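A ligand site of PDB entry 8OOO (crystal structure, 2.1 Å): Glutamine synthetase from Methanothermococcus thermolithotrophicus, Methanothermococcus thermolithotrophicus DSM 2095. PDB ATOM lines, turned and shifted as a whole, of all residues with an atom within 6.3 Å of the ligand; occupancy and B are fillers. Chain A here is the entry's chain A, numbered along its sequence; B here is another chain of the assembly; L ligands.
The side-chain hydroxyl of Ser 191 lies within hydrogen-bond range of an oxygen (O4) of the ligand, 2.7 Å away.
An oxygen (O2) of the ligand lies within salt-bridge range of the guanidinium group (NE) of Arg 88 of chain B (2.8 Å).
NH2 of Arg 20 of chain B lies within salt-bridge range of O2 of the ligand.
The guanidinium group (NE) of Arg 174 lies within salt-bridge range of an oxygen (O4) of the ligand (2.8 Å).
An oxygen (O1) of the ligand is in salt-bridge range of the guanidinium group of Arg 175.
The backbone carbonyl oxygen (O) of Ser 191 lies within hydrogen-bond range of the backbone NH (N) of Ala 34 of chain B (3.0 Å).
NH1 of Arg 88 of chain B is in salt-bridge range of OD1 of Asp 172 (2.7 Å).
The guanidinium group (NH2) of Arg 20 of chain B is in salt-bridge range of the side-chain carboxylate (OE2) of Glu 165 (3.0 Å).
The guanidinium group of Arg 174 lies within salt-bridge range of the side-chain carboxylate of Asp 168.
The guanidinium group (NH2) of Arg 175 lies within hydrogen-bond range of the backbone carbonyl oxygen (O) of Lys 92 of chain B, 2.7 Å away.
The backbone carbonyl oxygen (O) of Val 94 of chain B is in hydrogen-bond range of the backbone NH (N) of Leu 85 of chain B (2.8 Å).
CA of Pro 171 touches O5 of the ligand, at 3.5 Å.
Phe 18 of chain B touches the ligand.
Ala 34 of chain B touches the ligand.
Val 94 of chain B touches the ligand.
Hydrophobic or aromatic side chains that line the ligand: Pro 171, Phe 18 of chain B, Ala 34 of chain B and Val 94 of chain B.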
ATOM      1  N   GLU A 165       6.883  21.345  11.561  1.00  0.00           N
ATOM      2  CA  GLU A 165       6.380  19.993  11.773  1.00  0.00           C
ATOM      3  C   GLU A 165       7.555  19.151  12.300  1.00  0.00           C
ATOM      4  O   GLU A 165       8.722  19.478  12.007  1.00  0.00           O
ATOM      5  CB  GLU A 165       5.872  19.421  10.427  1.00  0.00           C
ATOM      6  CG  GLU A 165       6.904  19.520   9.297  1.00  0.00           C
ATOM      7  CD  GLU A 165       6.709  20.703   8.363  1.00  0.00           C
ATOM      8  OE1 GLU A 165       6.728  21.855   8.856  1.00  0.00           O
ATOM      9  OE2 GLU A 165       6.507  20.471   7.152  1.00  0.00           O
ATOM     10  N   ASP A 168       4.497  21.449  14.930  1.00  0.00           N
ATOM     11  CA  ASP A 168       3.417  22.166  14.283  1.00  0.00           C
ATOM     12  C   ASP A 168       2.681  21.082  13.488  1.00  0.00           C
ATOM     13  O   ASP A 168       3.250  20.524  12.551  1.00  0.00           O
ATOM     14  CB  ASP A 168       3.987  23.254  13.372  1.00  0.00           C
ATOM     15  CG  ASP A 168       3.039  23.759  12.308  1.00  0.00           C
ATOM     16  OD1 ASP A 168       1.799  23.787  12.571  1.00  0.00           O
ATOM     17  OD2 ASP A 168       3.531  24.147  11.219  1.00  0.00           O
ATOM     18  N   ALA A 170      -0.259  21.517  11.815  1.00  0.00           N
ATOM     19  CA  ALA A 170      -1.265  22.073  10.923  1.00  0.00           C
ATOM     20  C   ALA A 170      -0.808  22.453   9.503  1.00  0.00           C
ATOM     21  O   ALA A 170      -1.634  23.034   8.823  1.00  0.00           O
ATOM     22  CB  ALA A 170      -1.909  23.272  11.592  1.00  0.00           C
ATOM     23  N   PRO A 171       0.388  22.119   8.963  1.00  0.00           N
ATOM     24  CA  PRO A 171       0.665  22.518   7.569  1.00  0.00           C
ATOM     25  C   PRO A 171      -0.427  22.088   6.570  1.00  0.00           C
ATOM     26  O   PRO A 171      -0.780  22.876   5.699  1.00  0.00           O
ATOM     27  CB  PRO A 171       2.022  21.902   7.275  1.00  0.00           C
ATOM     28  CG  PRO A 171       2.676  21.797   8.632  1.00  0.00           C
ATOM     29  CD  PRO A 171       1.549  21.449   9.565  1.00  0.00           C
ATOM     30  N   ASP A 172      -0.981  20.885   6.704  1.00  0.00           N
ATOM     31  CA  ASP A 172      -2.039  20.418   5.796  1.00  0.00           C
ATOM     32  C   ASP A 172      -3.325  21.279   5.926  1.00  0.00           C
ATOM     33  O   ASP A 172      -3.985  21.533   4.924  1.00  0.00           O
ATOM     34  CB  ASP A 172      -2.401  18.958   6.081  1.00  0.00           C
ATOM     35  CG  ASP A 172      -1.413  17.950   5.519  1.00  0.00           C
ATOM     36  OD1 ASP A 172      -0.621  18.322   4.647  1.00  0.00           O
ATOM     37  OD2 ASP A 172      -1.462  16.764   5.941  1.00  0.00           O
ATOM     38  N   ARG A 174      -3.445  24.472   7.242  1.00  0.00           N
ATOM     39  CA  ARG A 174      -3.129  25.829   6.777  1.00  0.00           C
ATOM     40  C   ARG A 174      -3.008  25.885   5.235  1.00  0.00           C
ATOM     41  O   ARG A 174      -3.501  26.826   4.605  1.00  0.00           O
ATOM     42  CB  ARG A 174      -1.863  26.374   7.494  1.00  0.00           C
ATOM     43  CG  ARG A 174      -2.144  26.803   8.962  1.00  0.00           C
ATOM     44  CD  ARG A 174      -1.053  27.701   9.504  1.00  0.00           C
ATOM     45  NE  ARG A 174       0.259  27.153   9.175  1.00  0.00           N
ATOM     46  CZ  ARG A 174       0.919  26.265   9.925  1.00  0.00           C
ATOM     47  NH1 ARG A 174       0.428  25.878  11.089  1.00  0.00           N
ATOM     48  NH2 ARG A 174       2.095  25.795   9.525  1.00  0.00           N
ATOM     49  N   ARG A 175      -2.466  24.828   4.627  1.00  0.00           N
ATOM     50  CA  ARG A 175      -2.385  24.651   3.174  1.00  0.00           C
ATOM     51  C   ARG A 175      -3.777  24.753   2.519  1.00  0.00           C
ATOM     52  O   ARG A 175      -3.950  25.534   1.565  1.00  0.00           O
ATOM     53  CB  ARG A 175      -1.793  23.282   2.870  1.00  0.00           C
ATOM     54  CG  ARG A 175      -1.707  22.911   1.400  1.00  0.00           C
ATOM     55  CD  ARG A 175      -0.987  21.589   1.252  1.00  0.00           C
ATOM     56  NE  ARG A 175      -0.859  21.193  -0.131  1.00  0.00           N
ATOM     57  CZ  ARG A 175       0.199  21.420  -0.934  1.00  0.00           C
ATOM     58  NH1 ARG A 175       1.262  22.062  -0.466  1.00  0.00           N
ATOM     59  NH2 ARG A 175       0.185  20.999  -2.188  1.00  0.00           N
ATOM     60  N   ASP A 176      -4.740  23.945   2.987  1.00  0.00           N
ATOM     61  CA  ASP A 176      -6.079  23.931   2.437  1.00  0.00           C
ATOM     62  C   ASP A 176      -6.784  25.236   2.697  1.00  0.00           C
ATOM     63  O   ASP A 176      -7.539  25.686   1.844  1.00  0.00           O
ATOM     64  CB  ASP A 176      -6.903  22.777   3.013  1.00  0.00           C
ATOM     65  CG  ASP A 176      -6.473  21.418   2.471  1.00  0.00           C
ATOM     66  OD1 ASP A 176      -5.816  21.385   1.413  1.00  0.00           O
ATOM     67  OD2 ASP A 176      -6.823  20.400   3.097  1.00  0.00           O
ATOM     68  N   VAL A 178      -5.287  28.222   2.824  1.00  0.00           N
ATOM     69  CA  VAL A 178      -4.734  29.138   1.819  1.00  0.00           C
ATOM     70  C   VAL A 178      -5.342  28.875   0.434  1.00  0.00           C
ATOM     71  O   VAL A 178      -5.668  29.814  -0.260  1.00  0.00           O
ATOM     72  CB  VAL A 178      -3.187  29.011   1.779  1.00  0.00           C
ATOM     73  CG1 VAL A 178      -2.595  29.697   0.541  1.00  0.00           C
ATOM     74  CG2 VAL A 178      -2.570  29.540   3.084  1.00  0.00           C
ATOM     75  N   ALA A 190       0.866  35.163   4.064  1.00  0.00           N
ATOM     76  CA  ALA A 190       1.705  34.277   4.869  1.00  0.00           C
ATOM     77  C   ALA A 190       0.857  33.419   5.801  1.00  0.00           C
ATOM     78  O   ALA A 190      -0.298  33.745   6.078  1.00  0.00           O
ATOM     79  CB  ALA A 190       2.677  35.117   5.711  1.00  0.00           C
ATOM     80  N   SER A 191       1.431  32.288   6.263  1.00  0.00           N
ATOM     81  CA  SER A 191       0.713  31.463   7.234  1.00  0.00           C
ATOM     82  C   SER A 191       1.730  30.831   8.138  1.00  0.00           C
ATOM     83  O   SER A 191       2.865  30.552   7.746  1.00  0.00           O
ATOM     84  CB  SER A 191      -0.206  30.446   6.570  1.00  0.00           C
ATOM     85  OG  SER A 191       0.419  29.685   5.557  1.00  0.00           O
ATOM     86  N   HIS A 192       1.352  30.674   9.402  1.00  0.00           N
ATOM     87  CA  HIS A 192       2.294  30.110  10.366  1.00  0.00           C
ATOM     88  C   HIS A 192       1.606  29.763  11.653  1.00  0.00           C
ATOM     89  O   HIS A 192       0.527  30.248  11.930  1.00  0.00           O
ATOM     90  CB  HIS A 192       3.451  31.100  10.652  1.00  0.00           C
ATOM     91  CG  HIS A 192       2.970  32.417  11.195  1.00  0.00           C
ATOM     92  ND1 HIS A 192       2.746  32.590  12.552  1.00  0.00           N
ATOM     93  CD2 HIS A 192       2.643  33.554  10.547  1.00  0.00           C
ATOM     94  CE1 HIS A 192       2.270  33.823  12.681  1.00  0.00           C
ATOM     95  NE2 HIS A 192       2.185  34.441  11.513  1.00  0.00           N
ATOM     96  N   HIS A 193       2.245  28.899  12.437  1.00  0.00           N
ATOM     97  CA  HIS A 193       1.770  28.561  13.766  1.00  0.00           C
ATOM     98  C   HIS A 193       1.979  29.833  14.629  1.00  0.00           C
ATOM     99  O   HIS A 193       2.971  30.563  14.453  1.00  0.00           O
ATOM    100  CB  HIS A 193       2.567  27.365  14.319  1.00  0.00           C
ATOM    101  CG  HIS A 193       1.909  26.687  15.472  1.00  0.00           C
ATOM    102  ND1 HIS A 193       1.601  27.367  16.636  1.00  0.00           N
ATOM    103  CD2 HIS A 193       1.522  25.401  15.607  1.00  0.00           C
ATOM    104  CE1 HIS A 193       1.025  26.484  17.432  1.00  0.00           C
ATOM    105  NE2 HIS A 193       0.922  25.304  16.842  1.00  0.00           N
ATOM    106  N   GLU A 201      -2.171  31.552  12.226  1.00  0.00           N
ATOM    107  CA  GLU A 201      -2.414  32.827  11.586  1.00  0.00           C
ATOM    108  C   GLU A 201      -2.251  32.660  10.085  1.00  0.00           C
ATOM    109  O   GLU A 201      -1.323  31.978   9.625  1.00  0.00           O
ATOM    110  CB  GLU A 201      -1.434  33.888  12.107  1.00  0.00           C
ATOM    111  CG  GLU A 201      -1.836  35.285  11.672  1.00  0.00           C
ATOM    112  CD  GLU A 201      -1.075  36.426  12.308  1.00  0.00           C
ATOM    113  OE1 GLU A 201      -0.596  36.266  13.454  1.00  0.00           O
ATOM    114  OE2 GLU A 201      -0.974  37.479  11.651  1.00  0.00           O
ATOM    115  N   PHE B  18       4.556  26.838  -2.223  1.00  0.00           N
ATOM    116  CA  PHE B  18       4.867  27.488  -0.946  1.00  0.00           C
ATOM    117  C   PHE B  18       6.362  27.610  -0.753  1.00  0.00           C
ATOM    118  O   PHE B  18       7.122  26.708  -1.120  1.00  0.00           O
ATOM    119  CB  PHE B  18       4.294  26.684   0.229  1.00  0.00           C
ATOM    120  CG  PHE B  18       2.789  26.632   0.243  1.00  0.00           C
ATOM    121  CD1 PHE B  18       2.056  27.653   0.836  1.00  0.00           C
ATOM    122  CD2 PHE B  18       2.108  25.561  -0.317  1.00  0.00           C
ATOM    123  CE1 PHE B  18       0.646  27.625   0.830  1.00  0.00           C
ATOM    124  CE2 PHE B  18       0.696  25.526  -0.291  1.00  0.00           C
ATOM    125  CZ  PHE B  18      -0.018  26.577   0.263  1.00  0.00           C
ATOM    126  N   MET B  19       6.795  28.702  -0.143  1.00  0.00           N
ATOM    127  CA  MET B  19       8.200  28.890   0.199  1.00  0.00           C
ATOM    128  C   MET B  19       8.281  29.067   1.684  1.00  0.00           C
ATOM    129  O   MET B  19       7.698  30.013   2.197  1.00  0.00           O
ATOM    130  CB  MET B  19       8.766  30.129  -0.516  1.00  0.00           C
ATOM    131  CG  MET B  19      10.254  30.355  -0.246  1.00  0.00           C
ATOM    132  SD  MET B  19      11.297  29.091  -1.030  1.00  0.00           S
ATOM    133  CE  MET B  19      11.221  29.622  -2.783  1.00  0.00           C
ATOM    134  N   ARG B  20       8.953  28.161   2.396  1.00  0.00           N
ATOM    135  CA  ARG B  20       9.195  28.316   3.832  1.00  0.00           C
ATOM    136  C   ARG B  20      10.398  29.224   4.000  1.00  0.00           C
ATOM    137  O   ARG B  20      11.403  28.966   3.369  1.00  0.00           O
ATOM    138  CB  ARG B  20       9.514  26.969   4.511  1.00  0.00           C
ATOM    139  CG  ARG B  20       8.474  25.903   4.285  1.00  0.00           C
ATOM    140  CD  ARG B  20       7.153  26.186   5.001  1.00  0.00           C
ATOM    141  NE  ARG B  20       6.298  25.005   5.006  1.00  0.00           N
ATOM    142  CZ  ARG B  20       6.451  23.957   5.800  1.00  0.00           C
ATOM    143  NH1 ARG B  20       7.431  23.928   6.701  1.00  0.00           N
ATOM    144  NH2 ARG B  20       5.623  22.911   5.717  1.00  0.00           N
ATOM    145  N   VAL B  33       8.070  30.639   8.480  1.00  0.00           N
ATOM    146  CA  VAL B  33       6.805  31.218   8.062  1.00  0.00           C
ATOM    147  C   VAL B  33       6.648  30.755   6.596  1.00  0.00           C
ATOM    148  O   VAL B  33       7.659  30.656   5.875  1.00  0.00           O
ATOM    149  CB  VAL B  33       6.748  32.763   8.221  1.00  0.00           C
ATOM    150  CG1 VAL B  33       7.921  33.430   7.545  1.00  0.00           C
ATOM    151  CG2 VAL B  33       5.433  33.322   7.691  1.00  0.00           C
ATOM    152  N   ALA B  34       5.417  30.428   6.163  1.00  0.00           N
ATOM    153  CA  ALA B  34       5.202  29.978   4.792  1.00  0.00           C
ATOM    154  C   ALA B  34       4.651  31.109   3.912  1.00  0.00           C
ATOM    155  O   ALA B  34       3.672  31.743   4.285  1.00  0.00           O
ATOM    156  CB  ALA B  34       4.260  28.794   4.757  1.00  0.00           C
ATOM    157  N   PHE B  35       5.293  31.341   2.771  1.00  0.00           N
ATOM    158  CA  PHE B  35       4.841  32.355   1.814  1.00  0.00           C
ATOM    159  C   PHE B  35       4.151  31.603   0.644  1.00  0.00           C
ATOM    160  O   PHE B  35       4.778  30.744   0.008  1.00  0.00           O
ATOM    161  CB  PHE B  35       6.048  33.151   1.286  1.00  0.00           C
ATOM    162  CG  PHE B  35       5.728  34.064   0.130  1.00  0.00           C
ATOM    163  CD1 PHE B  35       5.158  35.305   0.343  1.00  0.00           C
ATOM    164  CD2 PHE B  35       5.965  33.663  -1.179  1.00  0.00           C
ATOM    165  CE1 PHE B  35       4.830  36.129  -0.732  1.00  0.00           C
ATOM    166  CE2 PHE B  35       5.660  34.508  -2.244  1.00  0.00           C
ATOM    167  CZ  PHE B  35       5.126  35.738  -2.015  1.00  0.00           C
ATOM    168  N   LEU B  85      10.847  20.340   0.111  1.00  0.00           N
ATOM    169  CA  LEU B  85      10.543  19.443   1.256  1.00  0.00           C
ATOM    170  C   LEU B  85       9.959  18.121   0.744  1.00  0.00           C
ATOM    171  O   LEU B  85       8.824  18.138   0.228  1.00  0.00           O
ATOM    172  CB  LEU B  85       9.573  20.149   2.206  1.00  0.00           C
ATOM    173  CG  LEU B  85      10.099  21.451   2.823  1.00  0.00           C
ATOM    174  CD1 LEU B  85       9.475  21.688   4.183  1.00  0.00           C
ATOM    175  CD2 LEU B  85      11.613  21.437   2.921  1.00  0.00           C
ATOM    176  N   ARG B  88       6.414  16.877   2.162  1.00  0.00           N
ATOM    177  CA  ARG B  88       5.251  17.672   1.660  1.00  0.00           C
ATOM    178  C   ARG B  88       4.795  17.171   0.288  1.00  0.00           C
ATOM    179  O   ARG B  88       5.567  16.466  -0.383  1.00  0.00           O
ATOM    180  CB  ARG B  88       5.608  19.157   1.628  1.00  0.00           C
ATOM    181  CG  ARG B  88       5.921  19.743   3.002  1.00  0.00           C
ATOM    182  CD  ARG B  88       4.932  19.279   4.041  1.00  0.00           C
ATOM    183  NE  ARG B  88       3.644  19.934   3.887  1.00  0.00           N
ATOM    184  CZ  ARG B  88       2.476  19.359   4.113  1.00  0.00           C
ATOM    185  NH1 ARG B  88       1.360  20.050   3.950  1.00  0.00           N
ATOM    186  NH2 ARG B  88       2.413  18.096   4.506  1.00  0.00           N
ATOM    187  N   PRO B  89       3.551  17.500  -0.149  1.00  0.00           N
ATOM    188  CA  PRO B  89       3.025  17.075  -1.457  1.00  0.00           C
ATOM    189  C   PRO B  89       3.901  17.387  -2.675  1.00  0.00           C
ATOM    190  O   PRO B  89       4.591  18.384  -2.680  1.00  0.00           O
ATOM    191  CB  PRO B  89       1.727  17.888  -1.575  1.00  0.00           C
ATOM    192  CG  PRO B  89       1.298  18.101  -0.148  1.00  0.00           C
ATOM    193  CD  PRO B  89       2.587  18.293   0.607  1.00  0.00           C
ATOM    194  N   LYS B  92       2.152  21.020  -6.498  1.00  0.00           N
ATOM    195  CA  LYS B  92       1.996  22.240  -5.708  1.00  0.00           C
ATOM    196  C   LYS B  92       2.898  22.060  -4.473  1.00  0.00           C
ATOM    197  O   LYS B  92       2.443  22.051  -3.327  1.00  0.00           O
ATOM    198  CB  LYS B  92       0.558  22.456  -5.297  1.00  0.00           C
ATOM    199  CG  LYS B  92      -0.376  22.580  -6.464  1.00  0.00           C
ATOM    200  CD  LYS B  92      -1.682  23.249  -5.995  1.00  0.00           C
ATOM    201  CE  LYS B  92      -2.717  23.349  -7.083  1.00  0.00           C
ATOM    202  NZ  LYS B  92      -4.062  23.638  -6.513  1.00  0.00           N
ATOM    203  N   VAL B  94       6.342  22.239  -1.820  1.00  0.00           N
ATOM    204  CA  VAL B  94       6.769  23.172  -0.813  1.00  0.00           C
ATOM    205  C   VAL B  94       8.277  23.214  -0.854  1.00  0.00           C
ATOM    206  O   VAL B  94       8.917  22.182  -0.755  1.00  0.00           O
ATOM    207  CB  VAL B  94       6.245  22.705   0.569  1.00  0.00           C
ATOM    208  CG1 VAL B  94       6.655  23.670   1.691  1.00  0.00           C
ATOM    209  CG2 VAL B  94       4.741  22.517   0.539  1.00  0.00           C
HETATM  210  C1  LIG L   1       2.702  23.316   3.195  1.00  0.00           C
HETATM  211  O1  LIG L   1       1.967  22.735   2.389  1.00  0.00           O
HETATM  212  O2  LIG L   1       3.664  22.708   3.696  1.00  0.00           O
HETATM  213  C2  LIG L   1       2.475  24.717   3.526  1.00  0.00           C
HETATM  214  O3  LIG L   1       3.451  25.451   3.564  1.00  0.00           O
HETATM  215  C3  LIG L   1       1.097  25.307   3.834  1.00  0.00           C
HETATM  216  C4  LIG L   1       1.189  26.699   4.495  1.00  0.00           C
HETATM  217  C5  LIG L   1       1.678  26.591   5.940  1.00  0.00           C
HETATM  218  O4  LIG L   1       1.624  27.575   6.714  1.00  0.00           O
HETATM  219  O5  LIG L   1       2.121  25.510   6.371  1.00  0.00           O
